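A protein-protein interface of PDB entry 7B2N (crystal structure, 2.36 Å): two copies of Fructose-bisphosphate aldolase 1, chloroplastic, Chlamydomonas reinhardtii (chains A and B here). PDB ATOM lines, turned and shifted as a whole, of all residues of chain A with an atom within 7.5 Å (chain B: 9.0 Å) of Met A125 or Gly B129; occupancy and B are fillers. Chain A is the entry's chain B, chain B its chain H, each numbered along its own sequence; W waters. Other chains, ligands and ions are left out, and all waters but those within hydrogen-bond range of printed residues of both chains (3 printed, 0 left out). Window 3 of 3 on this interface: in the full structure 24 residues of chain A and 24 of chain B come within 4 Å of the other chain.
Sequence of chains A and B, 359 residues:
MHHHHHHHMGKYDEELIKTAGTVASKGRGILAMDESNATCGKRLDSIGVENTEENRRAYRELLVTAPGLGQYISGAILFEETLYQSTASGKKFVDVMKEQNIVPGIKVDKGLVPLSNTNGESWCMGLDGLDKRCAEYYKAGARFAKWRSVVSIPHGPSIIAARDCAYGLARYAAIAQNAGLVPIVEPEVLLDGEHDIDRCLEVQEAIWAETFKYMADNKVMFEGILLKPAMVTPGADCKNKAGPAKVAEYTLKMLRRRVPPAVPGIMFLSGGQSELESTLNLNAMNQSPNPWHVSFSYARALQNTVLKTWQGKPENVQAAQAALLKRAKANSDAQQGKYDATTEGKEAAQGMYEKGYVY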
ATOM      1  N   VAL A 108     -14.408  13.334   0.830  1.00  0.00           N
ATOM      2  CA  VAL A 108     -14.255  12.250  -0.133  1.00  0.00           C
ATOM      3  C   VAL A 108     -12.813  11.805  -0.324  1.00  0.00           C
ATOM      4  O   VAL A 108     -12.584  10.793  -1.004  1.00  0.00           O
ATOM      5  CB  VAL A 108     -14.874  12.621  -1.497  1.00  0.00           C
ATOM      6  CG1 VAL A 108     -16.337  13.014  -1.325  1.00  0.00           C
ATOM      7  CG2 VAL A 108     -14.089  13.746  -2.142  1.00  0.00           C
ATOM      8  N   ASP A 109     -11.832  12.510   0.231  1.00  0.00           N
ATOM      9  CA  ASP A 109     -10.466  12.025   0.115  1.00  0.00           C
ATOM     10  C   ASP A 109     -10.234  10.884   1.105  1.00  0.00           C
ATOM     11  O   ASP A 109     -11.033  10.646   2.012  1.00  0.00           O
ATOM     12  CB  ASP A 109      -9.465  13.161   0.341  1.00  0.00           C
ATOM     13  CG  ASP A 109      -9.325  13.542   1.807  1.00  0.00           C
ATOM     14  OD1 ASP A 109      -8.652  12.807   2.556  1.00  0.00           O
ATOM     15  OD2 ASP A 109      -9.872  14.588   2.210  1.00  0.00           O
ATOM     16  N   LYS A 110      -9.113  10.180   0.932  1.00  0.00           N
ATOM     17  CA  LYS A 110      -8.786   9.021   1.756  1.00  0.00           C
ATOM     18  C   LYS A 110      -7.545   9.242   2.619  1.00  0.00           C
ATOM     19  O   LYS A 110      -6.912   8.273   3.046  1.00  0.00           O
ATOM     20  CB  LYS A 110      -8.614   7.775   0.884  1.00  0.00           C
ATOM     21  CG  LYS A 110      -9.919   7.017   0.625  1.00  0.00           C
ATOM     22  CD  LYS A 110     -10.096   6.684  -0.854  1.00  0.00           C
ATOM     23  CE  LYS A 110      -9.764   5.224  -1.160  1.00  0.00           C
ATOM     24  NZ  LYS A 110      -9.864   4.908  -2.624  1.00  0.00           N
ATOM     25  N   GLY A 111      -7.184  10.495   2.885  1.00  0.00           N
ATOM     26  CA  GLY A 111      -6.158  10.806   3.857  1.00  0.00           C
ATOM     27  C   GLY A 111      -4.763  10.938   3.265  1.00  0.00           C
ATOM     28  O   GLY A 111      -4.502  10.636   2.097  1.00  0.00           O
ATOM     29  N   LEU A 112      -3.848  11.394   4.115  1.00  0.00           N
ATOM     30  CA  LEU A 112      -2.468  11.652   3.736  1.00  0.00           C
ATOM     31  C   LEU A 112      -1.620  10.392   3.864  1.00  0.00           C
ATOM     32  O   LEU A 112      -1.828   9.563   4.754  1.00  0.00           O
ATOM     33  CB  LEU A 112      -1.876  12.764   4.603  1.00  0.00           C
ATOM     34  CG  LEU A 112      -2.677  14.064   4.650  1.00  0.00           C
ATOM     35  CD1 LEU A 112      -1.937  15.108   5.468  1.00  0.00           C
ATOM     36  CD2 LEU A 112      -2.953  14.580   3.242  1.00  0.00           C
ATOM     37  N   VAL A 113      -0.660  10.258   2.953  1.00  0.00           N
ATOM     38  CA  VAL A 113       0.211   9.089   2.834  1.00  0.00           C
ATOM     39  C   VAL A 113       1.601   9.605   2.481  1.00  0.00           C
ATOM     40  O   VAL A 113       1.709  10.609   1.763  1.00  0.00           O
ATOM     41  CB  VAL A 113      -0.304   8.109   1.762  1.00  0.00           C
ATOM     42  CG1 VAL A 113       0.474   6.802   1.790  1.00  0.00           C
ATOM     43  CG2 VAL A 113      -1.797   7.832   1.932  1.00  0.00           C
ATOM     44  N   TRP A 123       1.229  13.028   0.400  1.00  0.00           N
ATOM     45  CA  TRP A 123       0.255  13.274  -0.650  1.00  0.00           C
ATOM     46  C   TRP A 123      -1.092  12.752  -0.171  1.00  0.00           C
ATOM     47  O   TRP A 123      -1.179  11.968   0.780  1.00  0.00           O
ATOM     48  CB  TRP A 123       0.647  12.615  -1.983  1.00  0.00           C
ATOM     49  CG  TRP A 123       0.635  11.108  -1.971  1.00  0.00           C
ATOM     50  CD1 TRP A 123       1.518  10.286  -1.330  1.00  0.00           C
ATOM     51  CD2 TRP A 123      -0.296  10.247  -2.646  1.00  0.00           C
ATOM     52  NE1 TRP A 123       1.192   8.970  -1.559  1.00  0.00           N
ATOM     53  CE2 TRP A 123       0.082   8.919  -2.360  1.00  0.00           C
ATOM     54  CE3 TRP A 123      -1.413  10.470  -3.459  1.00  0.00           C
ATOM     55  CZ2 TRP A 123      -0.617   7.819  -2.862  1.00  0.00           C
ATOM     56  CZ3 TRP A 123      -2.104   9.374  -3.958  1.00  0.00           C
ATOM     57  CH2 TRP A 123      -1.703   8.068  -3.657  1.00  0.00           C
ATOM     58  N   CYS A 124      -2.149  13.201  -0.836  1.00  0.00           N
ATOM     59  CA  CYS A 124      -3.517  12.864  -0.464  1.00  0.00           C
ATOM     60  C   CYS A 124      -4.079  11.875  -1.479  1.00  0.00           C
ATOM     61  O   CYS A 124      -4.110  12.162  -2.681  1.00  0.00           O
ATOM     62  CB  CYS A 124      -4.374  14.126  -0.396  1.00  0.00           C
ATOM     63  SG  CYS A 124      -6.133  13.820  -0.215  1.00  0.00           S
ATOM     64  N   MET A 125      -4.518  10.718  -0.997  1.00  0.00           N
ATOM     65  CA  MET A 125      -5.061   9.652  -1.827  1.00  0.00           C
ATOM     66  C   MET A 125      -6.586   9.717  -1.874  1.00  0.00           C
ATOM     67  O   MET A 125      -7.237  10.275  -0.985  1.00  0.00           O
ATOM     68  CB  MET A 125      -4.614   8.288  -1.291  1.00  0.00           C
ATOM     69  CG  MET A 125      -4.953   8.068   0.173  1.00  0.00           C
ATOM     70  SD  MET A 125      -5.102   6.331   0.643  1.00  0.00           S
ATOM     71  CE  MET A 125      -3.806   5.635  -0.323  1.00  0.00           C
ATOM     72  N   GLY A 126      -7.155   9.135  -2.928  1.00  0.00           N
ATOM     73  CA  GLY A 126      -8.600   9.041  -3.001  1.00  0.00           C
ATOM     74  C   GLY A 126      -9.215   8.958  -4.384  1.00  0.00           C
ATOM     75  O   GLY A 126     -10.421   8.723  -4.506  1.00  0.00           O
ATOM     76  N   LEU A 127      -8.415   9.142  -5.438  1.00  0.00           N
ATOM     77  CA  LEU A 127      -8.991   9.185  -6.780  1.00  0.00           C
ATOM     78  C   LEU A 127      -9.598   7.846  -7.186  1.00  0.00           C
ATOM     79  O   LEU A 127     -10.547   7.815  -7.979  1.00  0.00           O
ATOM     80  CB  LEU A 127      -7.935   9.621  -7.796  1.00  0.00           C
ATOM     81  CG  LEU A 127      -7.339  11.012  -7.576  1.00  0.00           C
ATOM     82  CD1 LEU A 127      -6.252  11.313  -8.605  1.00  0.00           C
ATOM     83  CD2 LEU A 127      -8.426  12.070  -7.615  1.00  0.00           C
ATOM     84  N   ASP A 128      -9.076   6.739  -6.658  1.00  0.00           N
ATOM     85  CA  ASP A 128      -9.578   5.417  -7.021  1.00  0.00           C
ATOM     86  C   ASP A 128     -11.001   5.232  -6.505  1.00  0.00           C
ATOM     87  O   ASP A 128     -11.251   5.338  -5.300  1.00  0.00           O
ATOM     88  CB  ASP A 128      -8.660   4.336  -6.460  1.00  0.00           C
ATOM     89  CG  ASP A 128      -7.283   4.354  -7.094  1.00  0.00           C
ATOM     90  OD1 ASP A 128      -7.142   4.938  -8.189  1.00  0.00           O
ATOM     91  OD2 ASP A 128      -6.345   3.781  -6.497  1.00  0.00           O
ATOM     92  N   ARG A 133     -18.072   6.811  -5.762  1.00  0.00           N
ATOM     93  CA  ARG A 133     -18.330   7.254  -4.393  1.00  0.00           C
ATOM     94  C   ARG A 133     -19.119   8.558  -4.374  1.00  0.00           C
ATOM     95  O   ARG A 133     -20.128   8.671  -3.666  1.00  0.00           O
ATOM     96  CB  ARG A 133     -17.010   7.394  -3.634  1.00  0.00           C
ATOM     97  CG  ARG A 133     -16.769   6.296  -2.612  1.00  0.00           C
ATOM     98  CD  ARG A 133     -15.295   6.014  -2.355  1.00  0.00           C
ATOM     99  NE  ARG A 133     -14.538   7.192  -1.931  1.00  0.00           N
ATOM    100  CZ  ARG A 133     -13.371   7.558  -2.463  1.00  0.00           C
ATOM    101  NH1 ARG A 133     -12.825   6.845  -3.438  1.00  0.00           N
ATOM    102  NH2 ARG A 133     -12.746   8.641  -2.025  1.00  0.00           N
ATOM    103  N   TRP A 147     -11.807  17.833  -0.219  1.00  0.00           N
ATOM    104  CA  TRP A 147     -10.580  17.073  -0.413  1.00  0.00           C
ATOM    105  C   TRP A 147      -9.458  17.926   0.152  1.00  0.00           C
ATOM    106  O   TRP A 147      -9.308  19.084  -0.245  1.00  0.00           O
ATOM    107  CB  TRP A 147     -10.373  16.763  -1.900  1.00  0.00           C
ATOM    108  CG  TRP A 147      -9.051  16.166  -2.323  1.00  0.00           C
ATOM    109  CD1 TRP A 147      -7.825  16.771  -2.303  1.00  0.00           C
ATOM    110  CD2 TRP A 147      -8.845  14.864  -2.892  1.00  0.00           C
ATOM    111  NE1 TRP A 147      -6.868  15.919  -2.803  1.00  0.00           N
ATOM    112  CE2 TRP A 147      -7.468  14.745  -3.176  1.00  0.00           C
ATOM    113  CE3 TRP A 147      -9.688  13.789  -3.185  1.00  0.00           C
ATOM    114  CZ2 TRP A 147      -6.917  13.592  -3.731  1.00  0.00           C
ATOM    115  CZ3 TRP A 147      -9.140  12.643  -3.738  1.00  0.00           C
ATOM    116  CH2 TRP A 147      -7.766  12.555  -4.004  1.00  0.00           C
ATOM    117  N   ARG A 148      -8.708  17.380   1.103  1.00  0.00           N
ATOM    118  CA  ARG A 148      -7.658  18.124   1.780  1.00  0.00           C
ATOM    119  C   ARG A 148      -6.302  17.555   1.392  1.00  0.00           C
ATOM    120  O   ARG A 148      -6.019  16.380   1.652  1.00  0.00           O
ATOM    121  CB  ARG A 148      -7.830  18.092   3.297  1.00  0.00           C
ATOM    122  CG  ARG A 148      -6.640  18.689   4.040  1.00  0.00           C
ATOM    123  CD  ARG A 148      -6.934  18.860   5.518  1.00  0.00           C
ATOM    124  NE  ARG A 148      -5.768  19.340   6.255  1.00  0.00           N
ATOM    125  CZ  ARG A 148      -4.904  18.550   6.886  1.00  0.00           C
ATOM    126  NH1 ARG A 148      -5.065  17.234   6.875  1.00  0.00           N
ATOM    127  NH2 ARG A 148      -3.876  19.075   7.533  1.00  0.00           N
ATOM    128  N   SER A 149      -5.480  18.385   0.761  1.00  0.00           N
ATOM    129  CA  SER A 149      -4.075  18.106   0.515  1.00  0.00           C
ATOM    130  C   SER A 149      -3.260  19.169   1.230  1.00  0.00           C
ATOM    131  O   SER A 149      -3.793  20.196   1.658  1.00  0.00           O
ATOM    132  CB  SER A 149      -3.754  18.084  -0.985  1.00  0.00           C
ATOM    133  OG  SER A 149      -2.665  17.215  -1.254  1.00  0.00           O
ATOM    134  N   ASP A 164       1.823  17.137  -6.835  1.00  0.00           N
ATOM    135  CA  ASP A 164       0.769  16.143  -6.622  1.00  0.00           C
ATOM    136  C   ASP A 164      -0.424  16.735  -5.885  1.00  0.00           C
ATOM    137  O   ASP A 164      -1.572  16.359  -6.158  1.00  0.00           O
ATOM    138  CB  ASP A 164       1.303  14.934  -5.870  1.00  0.00           C
ATOM    139  CG  ASP A 164       0.322  13.783  -5.901  1.00  0.00           C
ATOM    140  OD1 ASP A 164       0.222  13.130  -6.960  1.00  0.00           O
ATOM    141  OD2 ASP A 164      -0.377  13.558  -4.886  1.00  0.00           O
ATOM    142  N   VAL B 108      -0.375  -4.809 -10.618  1.00  0.00           N
ATOM    143  CA  VAL B 108      -0.661  -3.991  -9.445  1.00  0.00           C
ATOM    144  C   VAL B 108      -1.608  -2.836  -9.733  1.00  0.00           C
ATOM    145  O   VAL B 108      -1.994  -2.130  -8.790  1.00  0.00           O
ATOM    146  CB  VAL B 108       0.636  -3.457  -8.799  1.00  0.00           C
ATOM    147  CG1 VAL B 108       1.561  -4.607  -8.412  1.00  0.00           C
ATOM    148  CG2 VAL B 108       1.335  -2.492  -9.733  1.00  0.00           C
ATOM    149  N   LYS B 110      -5.340  -1.139 -11.001  1.00  0.00           N
ATOM    150  CA  LYS B 110      -6.738  -1.474 -10.752  1.00  0.00           C
ATOM    151  C   LYS B 110      -7.620  -1.191 -11.965  1.00  0.00           C
ATOM    152  O   LYS B 110      -8.849  -1.158 -11.839  1.00  0.00           O
ATOM    153  CB  LYS B 110      -7.256  -0.741  -9.511  1.00  0.00           C
ATOM    154  CG  LYS B 110      -6.508  -1.097  -8.227  1.00  0.00           C
ATOM    155  CD  LYS B 110      -7.227  -0.587  -6.980  1.00  0.00           C
ATOM    156  CE  LYS B 110      -6.298   0.268  -6.116  1.00  0.00           C
ATOM    157  NZ  LYS B 110      -7.002   1.367  -5.391  1.00  0.00           N
ATOM    158  N   GLY B 126      -5.117   2.988  -9.465  1.00  0.00           N
ATOM    159  CA  GLY B 126      -4.335   2.069  -8.662  1.00  0.00           C
ATOM    160  C   GLY B 126      -3.402   2.626  -7.605  1.00  0.00           C
ATOM    161  O   GLY B 126      -2.845   1.853  -6.817  1.00  0.00           O
ATOM    162  N   LEU B 127      -3.212   3.945  -7.556  1.00  0.00           N
ATOM    163  CA  LEU B 127      -2.228   4.488  -6.622  1.00  0.00           C
ATOM    164  C   LEU B 127      -2.666   4.322  -5.172  1.00  0.00           C
ATOM    165  O   LEU B 127      -1.820   4.116  -4.292  1.00  0.00           O
ATOM    166  CB  LEU B 127      -1.955   5.959  -6.931  1.00  0.00           C
ATOM    167  CG  LEU B 127      -1.261   6.235  -8.267  1.00  0.00           C
ATOM    168  CD1 LEU B 127      -1.124   7.728  -8.505  1.00  0.00           C
ATOM    169  CD2 LEU B 127       0.095   5.543  -8.333  1.00  0.00           C
ATOM    170  N   ASP B 128      -3.968   4.403  -4.905  1.00  0.00           N
ATOM    171  CA  ASP B 128      -4.469   4.297  -3.542  1.00  0.00           C
ATOM    172  C   ASP B 128      -4.152   2.925  -2.961  1.00  0.00           C
ATOM    173  O   ASP B 128      -4.547   1.897  -3.520  1.00  0.00           O
ATOM    174  CB  ASP B 128      -5.974   4.553  -3.514  1.00  0.00           C
ATOM    175  CG  ASP B 128      -6.332   5.962  -3.941  1.00  0.00           C
ATOM    176  OD1 ASP B 128      -5.444   6.838  -3.905  1.00  0.00           O
ATOM    177  OD2 ASP B 128      -7.499   6.194  -4.319  1.00  0.00           O
ATOM    178  N   GLY B 129      -3.433   2.915  -1.841  1.00  0.00           N
ATOM    179  CA  GLY B 129      -3.026   1.688  -1.193  1.00  0.00           C
ATOM    180  C   GLY B 129      -1.940   0.905  -1.897  1.00  0.00           C
ATOM    181  O   GLY B 129      -1.564  -0.168  -1.406  1.00  0.00           O
ATOM    182  N   LEU B 130      -1.410   1.408  -3.017  1.00  0.00           N
ATOM    183  CA  LEU B 130      -0.453   0.628  -3.798  1.00  0.00           C
ATOM    184  C   LEU B 130       0.814   0.328  -3.002  1.00  0.00           C
ATOM    185  O   LEU B 130       1.392  -0.757  -3.132  1.00  0.00           O
ATOM    186  CB  LEU B 130      -0.108   1.363  -5.092  1.00  0.00           C
ATOM    187  CG  LEU B 130       0.897   0.659  -6.006  1.00  0.00           C
ATOM    188  CD1 LEU B 130       0.277  -0.582  -6.630  1.00  0.00           C
ATOM    189  CD2 LEU B 130       1.380   1.608  -7.076  1.00  0.00           C
ATOM    190  N   ASP B 131       1.261   1.274  -2.170  1.00  0.00           N
ATOM    191  CA  ASP B 131       2.473   1.045  -1.389  1.00  0.00           C
ATOM    192  C   ASP B 131       2.314  -0.155  -0.465  1.00  0.00           C
ATOM    193  O   ASP B 131       3.226  -0.982  -0.348  1.00  0.00           O
ATOM    194  CB  ASP B 131       2.846   2.303  -0.597  1.00  0.00           C
ATOM    195  CG  ASP B 131       1.809   2.671   0.454  1.00  0.00           C
ATOM    196  OD1 ASP B 131       0.615   2.369   0.252  1.00  0.00           O
ATOM    197  OD2 ASP B 131       2.190   3.268   1.482  1.00  0.00           O
ATOM    198  N   LYS B 132       1.154  -0.282   0.182  1.00  0.00           N
ATOM    199  CA  LYS B 132       0.932  -1.419   1.065  1.00  0.00           C
ATOM    200  C   LYS B 132       0.648  -2.697   0.286  1.00  0.00           C
ATOM    201  O   LYS B 132       0.999  -3.788   0.746  1.00  0.00           O
ATOM    202  CB  LYS B 132      -0.204  -1.111   2.040  1.00  0.00           C
ATOM    203  CG  LYS B 132       0.200  -0.106   3.118  1.00  0.00           C
ATOM    204  CD  LYS B 132      -0.990   0.394   3.920  1.00  0.00           C
ATOM    205  CE  LYS B 132      -0.541   1.004   5.243  1.00  0.00           C
ATOM    206  NZ  LYS B 132       0.892   1.438   5.217  1.00  0.00           N
ATOM    207  N   ARG B 133       0.051  -2.580  -0.901  1.00  0.00           N
ATOM    208  CA  ARG B 133      -0.221  -3.766  -1.713  1.00  0.00           C
ATOM    209  C   ARG B 133       1.061  -4.408  -2.243  1.00  0.00           C
ATOM    210  O   ARG B 133       1.182  -5.642  -2.247  1.00  0.00           O
ATOM    211  CB  ARG B 133      -1.156  -3.401  -2.859  1.00  0.00           C
ATOM    212  CG  ARG B 133      -2.439  -4.185  -2.848  1.00  0.00           C
ATOM    213  CD  ARG B 133      -3.574  -3.414  -3.463  1.00  0.00           C
ATOM    214  NE  ARG B 133      -3.272  -2.969  -4.817  1.00  0.00           N
ATOM    215  CZ  ARG B 133      -3.360  -1.705  -5.221  1.00  0.00           C
ATOM    216  NH1 ARG B 133      -3.734  -0.758  -4.371  1.00  0.00           N
ATOM    217  NH2 ARG B 133      -3.071  -1.386  -6.473  1.00  0.00           N
ATOM    218  N   CYS B 134       2.019  -3.583  -2.708  1.00  0.00           N
ATOM    219  CA  CYS B 134       3.293  -4.057  -3.250  1.00  0.00           C
ATOM    220  C   CYS B 134       4.209  -4.579  -2.156  1.00  0.00           C
ATOM    221  O   CYS B 134       5.018  -5.488  -2.401  1.00  0.00           O
ATOM    222  CB  CYS B 134       4.020  -2.941  -4.014  1.00  0.00           C
ATOM    223  SG  CYS B 134       3.281  -2.411  -5.568  1.00  0.00           S
ATOM    224  N   ALA B 135       4.138  -3.982  -0.956  1.00  0.00           N
ATOM    225  CA  ALA B 135       4.932  -4.451   0.172  1.00  0.00           C
ATOM    226  C   ALA B 135       4.574  -5.881   0.539  1.00  0.00           C
ATOM    227  O   ALA B 135       5.454  -6.657   0.930  1.00  0.00           O
ATOM    228  CB  ALA B 135       4.726  -3.519   1.358  1.00  0.00           C
ATOM    229  N   GLU B 136       3.300  -6.257   0.416  1.00  0.00           N
ATOM    230  CA  GLU B 136       2.913  -7.625   0.732  1.00  0.00           C
ATOM    231  C   GLU B 136       3.154  -8.569  -0.435  1.00  0.00           C
ATOM    232  O   GLU B 136       3.450  -9.747  -0.212  1.00  0.00           O
ATOM    233  CB  GLU B 136       1.450  -7.689   1.163  1.00  0.00           C
ATOM    234  CG  GLU B 136       1.184  -8.768   2.226  1.00  0.00           C
ATOM    235  CD  GLU B 136       0.917 -10.144   1.627  1.00  0.00           C
ATOM    236  OE1 GLU B 136       1.836 -10.995   1.610  1.00  0.00           O
ATOM    237  OE2 GLU B 136      -0.227 -10.379   1.180  1.00  0.00           O
ATOM    238  N   TYR B 137       3.024  -8.093  -1.675  1.00  0.00           N
ATOM    239  CA  TYR B 137       3.423  -8.917  -2.812  1.00  0.00           C
ATOM    240  C   TYR B 137       4.906  -9.259  -2.741  1.00  0.00           C
ATOM    241  O   TYR B 137       5.314 -10.368  -3.108  1.00  0.00           O
ATOM    242  CB  TYR B 137       3.109  -8.203  -4.124  1.00  0.00           C
ATOM    243  CG  TYR B 137       1.643  -7.940  -4.354  1.00  0.00           C
ATOM    244  CD1 TYR B 137       0.667  -8.716  -3.740  1.00  0.00           C
ATOM    245  CD2 TYR B 137       1.234  -6.914  -5.194  1.00  0.00           C
ATOM    246  CE1 TYR B 137      -0.673  -8.472  -3.956  1.00  0.00           C
ATOM    247  CE2 TYR B 137      -0.100  -6.664  -5.417  1.00  0.00           C
ATOM    248  CZ  TYR B 137      -1.050  -7.444  -4.798  1.00  0.00           C
ATOM    249  OH  TYR B 137      -2.381  -7.186  -5.029  1.00  0.00           O
ATOM    250  N   TRP B 147       1.970  -2.284 -14.528  1.00  0.00           N
ATOM    251  CA  TRP B 147       0.922  -1.269 -14.497  1.00  0.00           C
ATOM    252  C   TRP B 147       0.739  -0.784 -15.925  1.00  0.00           C
ATOM    253  O   TRP B 147       1.678  -0.248 -16.517  1.00  0.00           O
ATOM    254  CB  TRP B 147       1.311  -0.121 -13.552  1.00  0.00           C
ATOM    255  CG  TRP B 147       0.486   1.161 -13.604  1.00  0.00           C
ATOM    256  CD1 TRP B 147       0.316   1.997 -14.673  1.00  0.00           C
ATOM    257  CD2 TRP B 147      -0.225   1.768 -12.513  1.00  0.00           C
ATOM    258  NE1 TRP B 147      -0.469   3.069 -14.322  1.00  0.00           N
ATOM    259  CE2 TRP B 147      -0.816   2.951 -13.002  1.00  0.00           C
ATOM    260  CE3 TRP B 147      -0.431   1.414 -11.177  1.00  0.00           C
ATOM    261  CZ2 TRP B 147      -1.602   3.782 -12.201  1.00  0.00           C
ATOM    262  CZ3 TRP B 147      -1.212   2.240 -10.382  1.00  0.00           C
ATOM    263  CH2 TRP B 147      -1.787   3.410 -10.897  1.00  0.00           C
ATOM    264  N   ARG B 171       4.333   7.889 -10.996  1.00  0.00           N
ATOM    265  CA  ARG B 171       4.006   7.709  -9.581  1.00  0.00           C
ATOM    266  C   ARG B 171       4.147   6.243  -9.180  1.00  0.00           C
ATOM    267  O   ARG B 171       4.794   5.920  -8.176  1.00  0.00           O
ATOM    268  CB  ARG B 171       2.584   8.206  -9.278  1.00  0.00           C
ATOM    269  CG  ARG B 171       2.370   9.720  -9.345  1.00  0.00           C
ATOM    270  CD  ARG B 171       2.946  10.478  -8.144  1.00  0.00           C
ATOM    271  NE  ARG B 171       2.775   9.779  -6.872  1.00  0.00           N
ATOM    272  CZ  ARG B 171       1.675   9.826  -6.124  1.00  0.00           C
ATOM    273  NH1 ARG B 171       0.623  10.535  -6.515  1.00  0.00           N
ATOM    274  NH2 ARG B 171       1.622   9.156  -4.982  1.00  0.00           N
ATOM    275  N   ILE B 175       6.616   4.205  -6.419  1.00  0.00           N
ATOM    276  CA  ILE B 175       6.039   3.433  -5.321  1.00  0.00           C
ATOM    277  C   ILE B 175       6.548   1.998  -5.356  1.00  0.00           C
ATOM    278  O   ILE B 175       6.939   1.435  -4.327  1.00  0.00           O
ATOM    279  CB  ILE B 175       4.501   3.483  -5.375  1.00  0.00           C
ATOM    280  CG1 ILE B 175       3.990   4.890  -5.054  1.00  0.00           C
ATOM    281  CG2 ILE B 175       3.902   2.461  -4.423  1.00  0.00           C
ATOM    282  CD1 ILE B 175       2.558   5.132  -5.502  1.00  0.00           C
ATOM    283  N   ALA B 179       8.921  -0.242  -2.633  1.00  0.00           N
ATOM    284  CA  ALA B 179       8.412  -1.469  -2.035  1.00  0.00           C
ATOM    285  C   ALA B 179       9.253  -2.690  -2.386  1.00  0.00           C
ATOM    286  O   ALA B 179       9.012  -3.769  -1.835  1.00  0.00           O
ATOM    287  CB  ALA B 179       6.958  -1.705  -2.463  1.00  0.00           C
HETATM  288  O   HOH W   1      -5.367   8.727  -5.877  1.00  0.00           O
HETATM  289  O   HOH W   2      -4.896   6.514  -8.481  1.00  0.00           O
HETATM  290  O   HOH W   3       3.893   7.964  -3.487  1.00  0.00           O
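Lys A110 touches Asp B128, and with the chains exchanged Asp A128 touches Lys B110.
Gly A126 touches Asp B128, and with the chains exchanged Asp A128 touches Gly B126.
Leu A127 touches Asp B128, and with the chains exchanged Asp A128 touches Leu B127.
Asp A128 touches its own counterpart, Asp B128.
Positions printed for both chains: 108, 110, 126, 127, 128, 133 and 147.
Met A125 touches just these residues of chain B: Asp B128 and Gly B129.
No residue of chain B comes within 4 Å of Cys A124.
Of the printed residues of chain B, Gly A126 touches Asp B128.
Printed residues of chain B within 4 Å of Trp A123: Leu B127, Asp B128 and Arg B171.
Of the printed residues of chain B, Asp A164 touches Arg B171.
The nearest residue of chain B that does not touch Met A125 is Leu B127 (4.7 Å).
The side-chain carboxylate (OD2) of Asp B128 is in salt-bridge range of the side-chain amino group (NZ) of Lys A110 (3.2 Å).
The backbone NH (N) of Gly A126 is in hydrogen-bond range of the side-chain carboxylate (OD1) of Asp B128, 3.0 Å away.
The backbone NH (N) of Leu A127 sits at hydrogen-bond distance from the side-chain carboxylate (OD2) of Asp B128, at 3.3 Å.
The side-chain carboxylate of Asp A128 is in salt-bridge range of the side-chain amino group of Lys B110, 2.7 Å away.
OD1 of Asp A128 lies within hydrogen-bond range of N of Gly B126 (3.1 Å).
The backbone NH (N) of Leu B127 sits at hydrogen-bond distance from the side-chain carboxylate (OD2) of Asp A128 (3.3 Å).
OD2 of Asp B128 lies within hydrogen-bond range of N of Asp A128, at 2.9 Å.
The guanidinium group of Arg B171 lies within salt-bridge range of the side-chain carboxylate of Asp A164 (2.7 Å).
The indole nitrogen (NE1) of Trp A123 lies close to the guanidinium group (NH2) of Arg B171, at 3.5 Å.
Among the printed residues, merely in contact across the chains: Met A125 with Asp B128, Met A125 with Gly B129, Trp A123 with Leu B127, Val A113 with Asp B131 and Trp A123 with Asp B128.
NZ of Lys A110 is in hydrogen-bond range of O of Asp A128 (3.0 Å).
The backbone carbonyl oxygen of Gly A111 is in hydrogen-bond range of the backbone NH of Met A125 (3.1 Å).
The guanidinium group of Arg A133 is in hydrogen-bond range of the backbone carbonyl oxygen of Asp A128 (2.9 Å).
The side-chain amino group of Lys B110 lies within hydrogen-bond range of the backbone carbonyl oxygen of Asp B128 (3.1 Å).
The guanidinium group of Arg B133 is in hydrogen-bond range of the backbone carbonyl oxygen of Gly B126 (3.3 Å).
The backbone carbonyl oxygen (O) of Asp B128 sits at hydrogen-bond distance from the guanidinium group (NH1) of Arg B133.
Water W1 lies within hydrogen-bond range of the side-chain carboxylate (OD1) of Asp B128, the backbone NH (N) of Leu A127 and the backbone NH (N) of Gly A126.
Water W2 bridges the side-chain carboxylate (OD1) of Asp A128 (2.8 Å) and the backbone NH (N) of Leu B127 (3.2 Å).
Water W3 lies within hydrogen-bond range of the guanidinium group (NH2) of Arg B171 (3.0 Å) and the indole nitrogen (NE1) of Trp A123 (3.5 Å).
Of the 18 printed residues of chain B, 7 touch a printed residue of chain A.
Hydrophobic or aromatic side chains of chain B that line the printed part of chain A: Leu B127.
Among the printed residues, Asp or Glu carboxylates within 4 Å of a Lys or Arg side-chain nitrogen of the other chain: Lys A110 with Asp B128 (3.2 Å), Asp A128 with Lys B110 (2.7 Å) and Asp A164 with Arg B171 (2.7 Å).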
